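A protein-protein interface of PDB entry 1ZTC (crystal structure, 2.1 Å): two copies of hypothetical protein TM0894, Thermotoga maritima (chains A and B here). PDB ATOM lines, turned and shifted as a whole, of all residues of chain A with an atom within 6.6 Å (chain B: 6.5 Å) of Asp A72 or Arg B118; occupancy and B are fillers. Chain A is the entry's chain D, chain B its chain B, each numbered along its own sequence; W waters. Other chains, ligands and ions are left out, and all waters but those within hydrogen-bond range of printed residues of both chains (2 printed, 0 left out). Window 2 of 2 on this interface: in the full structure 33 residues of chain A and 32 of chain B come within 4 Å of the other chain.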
ATOM      1  N   PHE A  64      10.955  -4.334 -23.170  1.00  0.00           N
ATOM      2  CA  PHE A  64      11.927  -5.055 -22.360  1.00  0.00           C
ATOM      3  C   PHE A  64      13.342  -4.788 -22.862  1.00  0.00           C
ATOM      4  O   PHE A  64      14.280  -4.614 -22.078  1.00  0.00           O
ATOM      5  CB  PHE A  64      11.616  -6.555 -22.337  1.00  0.00           C
ATOM      6  CG  PHE A  64      10.708  -6.964 -21.209  1.00  0.00           C
ATOM      7  CD1 PHE A  64       9.404  -6.503 -21.154  1.00  0.00           C
ATOM      8  CD2 PHE A  64      11.161  -7.803 -20.191  1.00  0.00           C
ATOM      9  CE1 PHE A  64       8.545  -6.862 -20.121  1.00  0.00           C
ATOM     10  CE2 PHE A  64      10.313  -8.165 -19.143  1.00  0.00           C
ATOM     11  CZ  PHE A  64       8.992  -7.694 -19.121  1.00  0.00           C
ATOM     12  N   ILE A  69      16.064  -5.405 -19.672  1.00  0.00           N
ATOM     13  CA  ILE A  69      15.715  -6.500 -18.775  1.00  0.00           C
ATOM     14  C   ILE A  69      15.154  -7.689 -19.521  1.00  0.00           C
ATOM     15  O   ILE A  69      14.744  -7.585 -20.671  1.00  0.00           O
ATOM     16  CB  ILE A  69      14.692  -6.053 -17.711  1.00  0.00           C
ATOM     17  CG1 ILE A  69      13.455  -5.441 -18.364  1.00  0.00           C
ATOM     18  CG2 ILE A  69      15.331  -5.064 -16.728  1.00  0.00           C
ATOM     19  CD1 ILE A  69      12.259  -5.375 -17.436  1.00  0.00           C
ATOM     20  N   SER A  70      15.123  -8.821 -18.834  1.00  0.00           N
ATOM     21  CA  SER A  70      14.476 -10.012 -19.349  1.00  0.00           C
ATOM     22  C   SER A  70      13.267 -10.314 -18.465  1.00  0.00           C
ATOM     23  O   SER A  70      13.141  -9.770 -17.361  1.00  0.00           O
ATOM     24  CB  SER A  70      15.460 -11.187 -19.380  1.00  0.00           C
ATOM     25  OG  SER A  70      15.195 -12.150 -18.399  1.00  0.00           O
ATOM     26  N   PRO A  71      12.364 -11.171 -18.950  1.00  0.00           N
ATOM     27  CA  PRO A  71      11.291 -11.693 -18.113  1.00  0.00           C
ATOM     28  C   PRO A  71      11.780 -12.358 -16.801  1.00  0.00           C
ATOM     29  O   PRO A  71      11.090 -12.304 -15.785  1.00  0.00           O
ATOM     30  CB  PRO A  71      10.613 -12.712 -19.034  1.00  0.00           C
ATOM     31  CG  PRO A  71      10.867 -12.171 -20.403  1.00  0.00           C
ATOM     32  CD  PRO A  71      12.264 -11.669 -20.331  1.00  0.00           C
ATOM     33  N   ASP A  72      12.978 -12.938 -16.825  1.00  0.00           N
ATOM     34  CA  ASP A  72      13.570 -13.541 -15.648  1.00  0.00           C
ATOM     35  C   ASP A  72      13.851 -12.568 -14.500  1.00  0.00           C
ATOM     36  O   ASP A  72      14.064 -13.011 -13.366  1.00  0.00           O
ATOM     37  CB  ASP A  72      14.892 -14.231 -15.995  1.00  0.00           C
ATOM     38  CG  ASP A  72      14.709 -15.455 -16.876  1.00  0.00           C
ATOM     39  OD1 ASP A  72      13.634 -16.087 -16.833  1.00  0.00           O
ATOM     40  OD2 ASP A  72      15.658 -15.786 -17.607  1.00  0.00           O
ATOM     41  N   ASP A  73      13.892 -11.275 -14.805  1.00  0.00           N
ATOM     42  CA  ASP A  73      14.189 -10.240 -13.816  1.00  0.00           C
ATOM     43  C   ASP A  73      12.945  -9.710 -13.118  1.00  0.00           C
ATOM     44  O   ASP A  73      13.055  -8.949 -12.170  1.00  0.00           O
ATOM     45  CB  ASP A  73      14.900  -9.043 -14.469  1.00  0.00           C
ATOM     46  CG  ASP A  73      16.211  -9.424 -15.137  1.00  0.00           C
ATOM     47  OD1 ASP A  73      16.986 -10.188 -14.533  1.00  0.00           O
ATOM     48  OD2 ASP A  73      16.476  -8.940 -16.261  1.00  0.00           O
ATOM     49  N   ILE A  74      11.766 -10.072 -13.594  1.00  0.00           N
ATOM     50  CA  ILE A  74      10.533  -9.624 -12.959  1.00  0.00           C
ATOM     51  C   ILE A  74      10.343 -10.384 -11.646  1.00  0.00           C
ATOM     52  O   ILE A  74      10.373 -11.614 -11.629  1.00  0.00           O
ATOM     53  CB  ILE A  74       9.331  -9.809 -13.907  1.00  0.00           C
ATOM     54  CG1 ILE A  74       9.546  -8.987 -15.188  1.00  0.00           C
ATOM     55  CG2 ILE A  74       8.045  -9.472 -13.232  1.00  0.00           C
ATOM     56  CD1 ILE A  74       9.764  -7.494 -14.950  1.00  0.00           C
ATOM     57  N   THR A  75      10.173  -9.631 -10.558  1.00  0.00           N
ATOM     58  CA  THR A  75      10.094 -10.179  -9.206  1.00  0.00           C
ATOM     59  C   THR A  75       8.665 -10.340  -8.687  1.00  0.00           C
ATOM     60  O   THR A  75       8.393 -11.214  -7.862  1.00  0.00           O
ATOM     61  CB  THR A  75      10.866  -9.276  -8.184  1.00  0.00           C
ATOM     62  OG1 THR A  75      10.381  -7.919  -8.228  1.00  0.00           O
ATOM     63  CG2 THR A  75      12.354  -9.283  -8.478  1.00  0.00           C
ATOM     64  N   VAL A  91       2.728 -16.337 -17.841  1.00  0.00           N
ATOM     65  CA  VAL A  91       3.535 -17.540 -18.119  1.00  0.00           C
ATOM     66  C   VAL A  91       5.010 -17.233 -18.430  1.00  0.00           C
ATOM     67  O   VAL A  91       5.859 -18.122 -18.342  1.00  0.00           O
ATOM     68  CB  VAL A  91       2.948 -18.393 -19.264  1.00  0.00           C
ATOM     69  CG1 VAL A  91       1.520 -18.812 -18.947  1.00  0.00           C
ATOM     70  CG2 VAL A  91       3.040 -17.660 -20.626  1.00  0.00           C
ATOM     71  N   LEU A  92       5.313 -15.979 -18.765  1.00  0.00           N
ATOM     72  CA  LEU A  92       6.703 -15.567 -19.067  1.00  0.00           C
ATOM     73  C   LEU A  92       7.583 -15.391 -17.846  1.00  0.00           C
ATOM     74  O   LEU A  92       8.814 -15.424 -17.956  1.00  0.00           O
ATOM     75  CB  LEU A  92       6.707 -14.236 -19.822  1.00  0.00           C
ATOM     76  CG  LEU A  92       6.003 -14.225 -21.180  1.00  0.00           C
ATOM     77  CD1 LEU A  92       5.827 -12.774 -21.647  1.00  0.00           C
ATOM     78  CD2 LEU A  92       6.761 -15.035 -22.174  1.00  0.00           C
ATOM     79  N   PHE A  93       6.961 -15.185 -16.683  1.00  0.00           N
ATOM     80  CA  PHE A  93       7.704 -14.725 -15.508  1.00  0.00           C
ATOM     81  C   PHE A  93       7.888 -15.839 -14.490  1.00  0.00           C
ATOM     82  O   PHE A  93       7.097 -16.006 -13.572  1.00  0.00           O
ATOM     83  CB  PHE A  93       7.009 -13.500 -14.918  1.00  0.00           C
ATOM     84  CG  PHE A  93       6.728 -12.454 -15.946  1.00  0.00           C
ATOM     85  CD1 PHE A  93       7.771 -11.846 -16.615  1.00  0.00           C
ATOM     86  CD2 PHE A  93       5.447 -12.113 -16.271  1.00  0.00           C
ATOM     87  CE1 PHE A  93       7.523 -10.903 -17.610  1.00  0.00           C
ATOM     88  CE2 PHE A  93       5.198 -11.179 -17.244  1.00  0.00           C
ATOM     89  CZ  PHE A  93       6.256 -10.581 -17.925  1.00  0.00           C
ATOM     90  N   GLU A  94       8.956 -16.595 -14.669  1.00  0.00           N
ATOM     91  CA  GLU A  94       9.168 -17.816 -13.930  1.00  0.00           C
ATOM     92  C   GLU A  94       9.673 -17.565 -12.520  1.00  0.00           C
ATOM     93  O   GLU A  94       9.638 -18.463 -11.707  1.00  0.00           O
ATOM     94  CB  GLU A  94      10.239 -18.692 -14.601  1.00  0.00           C
ATOM     95  CG  GLU A  94      10.255 -18.705 -16.130  1.00  0.00           C
ATOM     96  CD  GLU A  94       9.633 -19.921 -16.743  1.00  0.00           C
ATOM     97  OE1 GLU A  94       9.632 -21.002 -16.106  1.00  0.00           O
ATOM     98  OE2 GLU A  94       9.174 -19.782 -17.897  1.00  0.00           O
ATOM     99  N   ASN A  95      10.195 -16.369 -12.262  1.00  0.00           N
ATOM    100  CA  ASN A  95      10.803 -16.044 -10.960  1.00  0.00           C
ATOM    101  C   ASN A  95       9.941 -15.116 -10.116  1.00  0.00           C
ATOM    102  O   ASN A  95      10.353 -14.723  -9.034  1.00  0.00           O
ATOM    103  CB  ASN A  95      12.162 -15.368 -11.135  1.00  0.00           C
ATOM    104  CG  ASN A  95      13.185 -16.264 -11.801  1.00  0.00           C
ATOM    105  OD1 ASN A  95      13.266 -17.451 -11.501  1.00  0.00           O
ATOM    106  ND2 ASN A  95      13.982 -15.690 -12.701  1.00  0.00           N
ATOM    107  N   ALA A  96       8.754 -14.773 -10.608  1.00  0.00           N
ATOM    108  CA  ALA A  96       7.924 -13.795  -9.943  1.00  0.00           C
ATOM    109  C   ALA A  96       7.053 -14.414  -8.863  1.00  0.00           C
ATOM    110  O   ALA A  96       6.662 -15.577  -8.940  1.00  0.00           O
ATOM    111  CB  ALA A  96       7.018 -13.058 -10.960  1.00  0.00           C
ATOM    112  N   TYR B 109      14.746 -21.421 -31.711  1.00  0.00           N
ATOM    113  CA  TYR B 109      13.522 -20.643 -31.447  1.00  0.00           C
ATOM    114  C   TYR B 109      13.709 -19.631 -30.312  1.00  0.00           C
ATOM    115  O   TYR B 109      13.068 -18.581 -30.334  1.00  0.00           O
ATOM    116  CB  TYR B 109      12.303 -21.576 -31.229  1.00  0.00           C
ATOM    117  CG  TYR B 109      11.882 -22.243 -32.530  1.00  0.00           C
ATOM    118  CD1 TYR B 109      11.048 -21.580 -33.421  1.00  0.00           C
ATOM    119  CD2 TYR B 109      12.373 -23.505 -32.894  1.00  0.00           C
ATOM    120  CE1 TYR B 109      10.670 -22.157 -34.625  1.00  0.00           C
ATOM    121  CE2 TYR B 109      11.998 -24.106 -34.100  1.00  0.00           C
ATOM    122  CZ  TYR B 109      11.153 -23.422 -34.968  1.00  0.00           C
ATOM    123  OH  TYR B 109      10.782 -23.968 -36.189  1.00  0.00           O
ATOM    124  N   LEU B 110      14.615 -19.921 -29.369  1.00  0.00           N
ATOM    125  CA  LEU B 110      14.975 -18.965 -28.301  1.00  0.00           C
ATOM    126  C   LEU B 110      15.697 -17.693 -28.803  1.00  0.00           C
ATOM    127  O   LEU B 110      15.773 -16.699 -28.070  1.00  0.00           O
ATOM    128  CB  LEU B 110      15.792 -19.659 -27.198  1.00  0.00           C
ATOM    129  CG  LEU B 110      14.997 -20.628 -26.299  1.00  0.00           C
ATOM    130  CD1 LEU B 110      15.942 -21.332 -25.322  1.00  0.00           C
ATOM    131  CD2 LEU B 110      13.855 -19.923 -25.532  1.00  0.00           C
ATOM    132  N   GLY B 113      13.700 -13.770 -29.920  1.00  0.00           N
ATOM    133  CA  GLY B 113      13.428 -12.678 -28.974  1.00  0.00           C
ATOM    134  C   GLY B 113      13.261 -13.270 -27.583  1.00  0.00           C
ATOM    135  O   GLY B 113      12.754 -14.388 -27.448  1.00  0.00           O
ATOM    136  N   THR B 114      13.665 -12.549 -26.541  1.00  0.00           N
ATOM    137  CA  THR B 114      13.508 -13.092 -25.191  1.00  0.00           C
ATOM    138  C   THR B 114      12.074 -13.574 -25.030  1.00  0.00           C
ATOM    139  O   THR B 114      11.847 -14.759 -24.802  1.00  0.00           O
ATOM    140  CB  THR B 114      13.823 -12.090 -24.036  1.00  0.00           C
ATOM    141  OG1 THR B 114      12.976 -10.935 -24.131  1.00  0.00           O
ATOM    142  CG2 THR B 114      15.280 -11.657 -24.035  1.00  0.00           C
ATOM    143  N   ILE B 115      11.113 -12.684 -25.243  1.00  0.00           N
ATOM    144  CA  ILE B 115       9.728 -12.989 -24.950  1.00  0.00           C
ATOM    145  C   ILE B 115       9.147 -13.980 -25.925  1.00  0.00           C
ATOM    146  O   ILE B 115       8.685 -15.036 -25.531  1.00  0.00           O
ATOM    147  CB  ILE B 115       8.927 -11.677 -24.865  1.00  0.00           C
ATOM    148  CG1 ILE B 115       9.286 -10.977 -23.555  1.00  0.00           C
ATOM    149  CG2 ILE B 115       7.454 -11.939 -24.969  1.00  0.00           C
ATOM    150  CD1 ILE B 115       8.917  -9.548 -23.494  1.00  0.00           C
ATOM    151  N   VAL B 116       9.185 -13.644 -27.202  1.00  0.00           N
ATOM    152  CA  VAL B 116       8.572 -14.462 -28.237  1.00  0.00           C
ATOM    153  C   VAL B 116       9.232 -15.865 -28.299  1.00  0.00           C
ATOM    154  O   VAL B 116       8.542 -16.862 -28.443  1.00  0.00           O
ATOM    155  CB  VAL B 116       8.631 -13.730 -29.626  1.00  0.00           C
ATOM    156  CG1 VAL B 116       8.116 -14.601 -30.734  1.00  0.00           C
ATOM    157  CG2 VAL B 116       7.850 -12.405 -29.582  1.00  0.00           C
ATOM    158  N   GLY B 117      10.550 -15.925 -28.152  1.00  0.00           N
ATOM    159  CA  GLY B 117      11.265 -17.196 -28.105  1.00  0.00           C
ATOM    160  C   GLY B 117      10.781 -18.104 -26.980  1.00  0.00           C
ATOM    161  O   GLY B 117      10.611 -19.296 -27.185  1.00  0.00           O
ATOM    162  N   ARG B 118      10.528 -17.532 -25.805  1.00  0.00           N
ATOM    163  CA  ARG B 118       9.999 -18.292 -24.673  1.00  0.00           C
ATOM    164  C   ARG B 118       8.642 -18.919 -24.969  1.00  0.00           C
ATOM    165  O   ARG B 118       8.391 -20.057 -24.592  1.00  0.00           O
ATOM    166  CB  ARG B 118       9.894 -17.406 -23.456  1.00  0.00           C
ATOM    167  CG  ARG B 118      11.216 -17.124 -22.831  1.00  0.00           C
ATOM    168  CD  ARG B 118      11.139 -15.889 -21.998  1.00  0.00           C
ATOM    169  NE  ARG B 118      12.465 -15.473 -21.541  1.00  0.00           N
ATOM    170  CZ  ARG B 118      13.036 -15.836 -20.391  1.00  0.00           C
ATOM    171  NH1 ARG B 118      12.423 -16.644 -19.526  1.00  0.00           N
ATOM    172  NH2 ARG B 118      14.240 -15.365 -20.103  1.00  0.00           N
ATOM    173  N   ILE B 119       7.782 -18.189 -25.660  1.00  0.00           N
ATOM    174  CA  ILE B 119       6.482 -18.726 -26.015  1.00  0.00           C
ATOM    175  C   ILE B 119       6.613 -19.878 -26.993  1.00  0.00           C
ATOM    176  O   ILE B 119       5.994 -20.916 -26.790  1.00  0.00           O
ATOM    177  CB  ILE B 119       5.517 -17.676 -26.603  1.00  0.00           C
ATOM    178  CG1 ILE B 119       5.289 -16.544 -25.626  1.00  0.00           C
ATOM    179  CG2 ILE B 119       4.169 -18.329 -26.930  1.00  0.00           C
ATOM    180  CD1 ILE B 119       4.585 -16.973 -24.332  1.00  0.00           C
ATOM    181  N   TYR B 120       7.390 -19.696 -28.056  1.00  0.00           N
ATOM    182  CA  TYR B 120       7.639 -20.787 -29.002  1.00  0.00           C
ATOM    183  C   TYR B 120       8.166 -22.017 -28.264  1.00  0.00           C
ATOM    184  O   TYR B 120       7.721 -23.130 -28.484  1.00  0.00           O
ATOM    185  CB  TYR B 120       8.649 -20.363 -30.089  1.00  0.00           C
ATOM    186  CG  TYR B 120       8.027 -19.693 -31.281  1.00  0.00           C
ATOM    187  CD1 TYR B 120       7.833 -18.326 -31.325  1.00  0.00           C
ATOM    188  CD2 TYR B 120       7.619 -20.447 -32.372  1.00  0.00           C
ATOM    189  CE1 TYR B 120       7.243 -17.729 -32.442  1.00  0.00           C
ATOM    190  CE2 TYR B 120       7.057 -19.878 -33.468  1.00  0.00           C
ATOM    191  CZ  TYR B 120       6.870 -18.517 -33.510  1.00  0.00           C
ATOM    192  OH  TYR B 120       6.277 -17.992 -34.632  1.00  0.00           O
ATOM    193  N   SER B 121       9.133 -21.798 -27.387  1.00  0.00           N
ATOM    194  CA  SER B 121       9.769 -22.885 -26.676  1.00  0.00           C
ATOM    195  C   SER B 121       8.766 -23.663 -25.806  1.00  0.00           C
ATOM    196  O   SER B 121       8.770 -24.895 -25.796  1.00  0.00           O
ATOM    197  CB  SER B 121      10.930 -22.340 -25.848  1.00  0.00           C
ATOM    198  OG  SER B 121      11.305 -23.302 -24.896  1.00  0.00           O
ATOM    199  N   LYS B 122       7.908 -22.951 -25.099  1.00  0.00           N
ATOM    200  CA  LYS B 122       6.869 -23.583 -24.275  1.00  0.00           C
ATOM    201  C   LYS B 122       5.840 -24.360 -25.105  1.00  0.00           C
ATOM    202  O   LYS B 122       5.436 -25.447 -24.754  1.00  0.00           O
ATOM    203  CB  LYS B 122       6.185 -22.537 -23.386  1.00  0.00           C
ATOM    204  CG  LYS B 122       7.062 -22.063 -22.217  1.00  0.00           C
ATOM    205  CD  LYS B 122       6.522 -20.777 -21.605  1.00  0.00           C
ATOM    206  CE  LYS B 122       7.429 -20.250 -20.460  1.00  0.00           C
ATOM    207  NZ  LYS B 122       7.493 -21.151 -19.277  1.00  0.00           N
ATOM    208  N   VAL B 123       5.434 -23.816 -26.236  1.00  0.00           N
ATOM    209  CA  VAL B 123       4.513 -24.548 -27.105  1.00  0.00           C
ATOM    210  C   VAL B 123       5.158 -25.817 -27.640  1.00  0.00           C
ATOM    211  O   VAL B 123       4.608 -26.910 -27.505  1.00  0.00           O
ATOM    212  CB  VAL B 123       4.032 -23.677 -28.271  1.00  0.00           C
ATOM    213  CG1 VAL B 123       3.239 -24.507 -29.277  1.00  0.00           C
ATOM    214  CG2 VAL B 123       3.202 -22.539 -27.744  1.00  0.00           C
HETATM  215  O   HOH W   1       5.334 -20.860 -17.580  1.00  0.00           O
HETATM  216  O   HOH W   2       9.855 -17.657 -19.435  1.00  0.00           O
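OD2 of Asp A72 is in salt-bridge range of NH2 of Arg B118, at 2.9 Å.
NZ of Lys B122 lies within salt-bridge range of OE2 of Glu A94, at 2.6 Å.
The backbone carbonyl oxygen of Thr B114 sits close to the guanidinium group of Arg B118, 3.4 Å away.
The backbone carbonyl oxygen of Phe A64 sits at hydrogen-bond distance from the backbone NH of Ile A69, 3.1 Å away.
The side-chain hydroxyl (OG) of Ser A70 sits at hydrogen-bond distance from the backbone NH (N) of Asp A72 (2.8 Å).
N of Ser A70 lies within hydrogen-bond range of OD2 of Asp A73 (2.9 Å).
The side-chain amide nitrogen (ND2) of Asn A95 sits at hydrogen-bond distance from the backbone carbonyl oxygen (O) of Asp A72, at 2.8 Å.
Among the printed residues, merely in contact across the chains: Val A91 with Lys B122 (3.4 Å), Leu A92 with Ile B119 (3.6 Å), Pro A71 with Ile B115 (3.7 Å), Ser A70 with Arg B118 (3.8 Å), Leu A92 with Ile B115 (3.8 Å), Pro A71 with Arg B118 (3.8 Å), Phe A64 with Ile B115 (3.9 Å) and Pro A71 with Thr B114 (3.9 Å).
Printed residues of chain B within 4 Å of Ser A70: Arg B118 (3.8 Å).
Asp A72 touches just one residue of chain B: Arg B118 (2.9 Å).
Leu B110 touches none of the printed residues of chain A.
Of the printed residues of chain A, Thr B114 touches Pro A71 (3.9 Å).
Of chain A, only Ser A70 (3.8 Å), Pro A71 (3.8 Å) and Asp A72 (2.9 Å) come within 4 Å of Arg B118.
Of the printed residues of chain A, Lys B122 touches Val A91 and Glu A94.
The nearest printed residue of chain B that does not touch Pro A71 is Val B116 (7.2 Å).
Of the 13 printed residues of chain B, 5 touch a printed residue of chain A.
Hydrophobic or aromatic side chains of chain B within 4 Å of the printed part of chain A: Ile B115 and Ile B119.
Of the 14 printed residues of chain A, 7 touch a printed residue of chain B.
Hydrophobic or aromatic side chains of chain A that line the printed part of chain B: Phe A64, Pro A71 and Leu A92.
Among the printed residues, Asp or Glu carboxylates within 4 Å of a Lys or Arg side-chain nitrogen of the other chain: Asp A72 with Arg B118 (2.9 Å) and Glu A94 with Lys B122 (2.6 Å).
No position is printed for both chains.
Of the 10 pairs that touch across the chains among the printed residues, none has its exchanged pair printed and touching as well.
Water W2 lies within hydrogen-bond range of the side-chain carboxylate (OE2) of Glu A94 (2.7 Å), the guanidinium group (NH1) of Arg B118 (2.8 Å) and the backbone carbonyl oxygen (O) of Leu A92 (2.9 Å).
Water W1 bridges the side-chain amino group (NZ) of Lys B122 and the backbone carbonyl oxygen (O) of Val A91.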
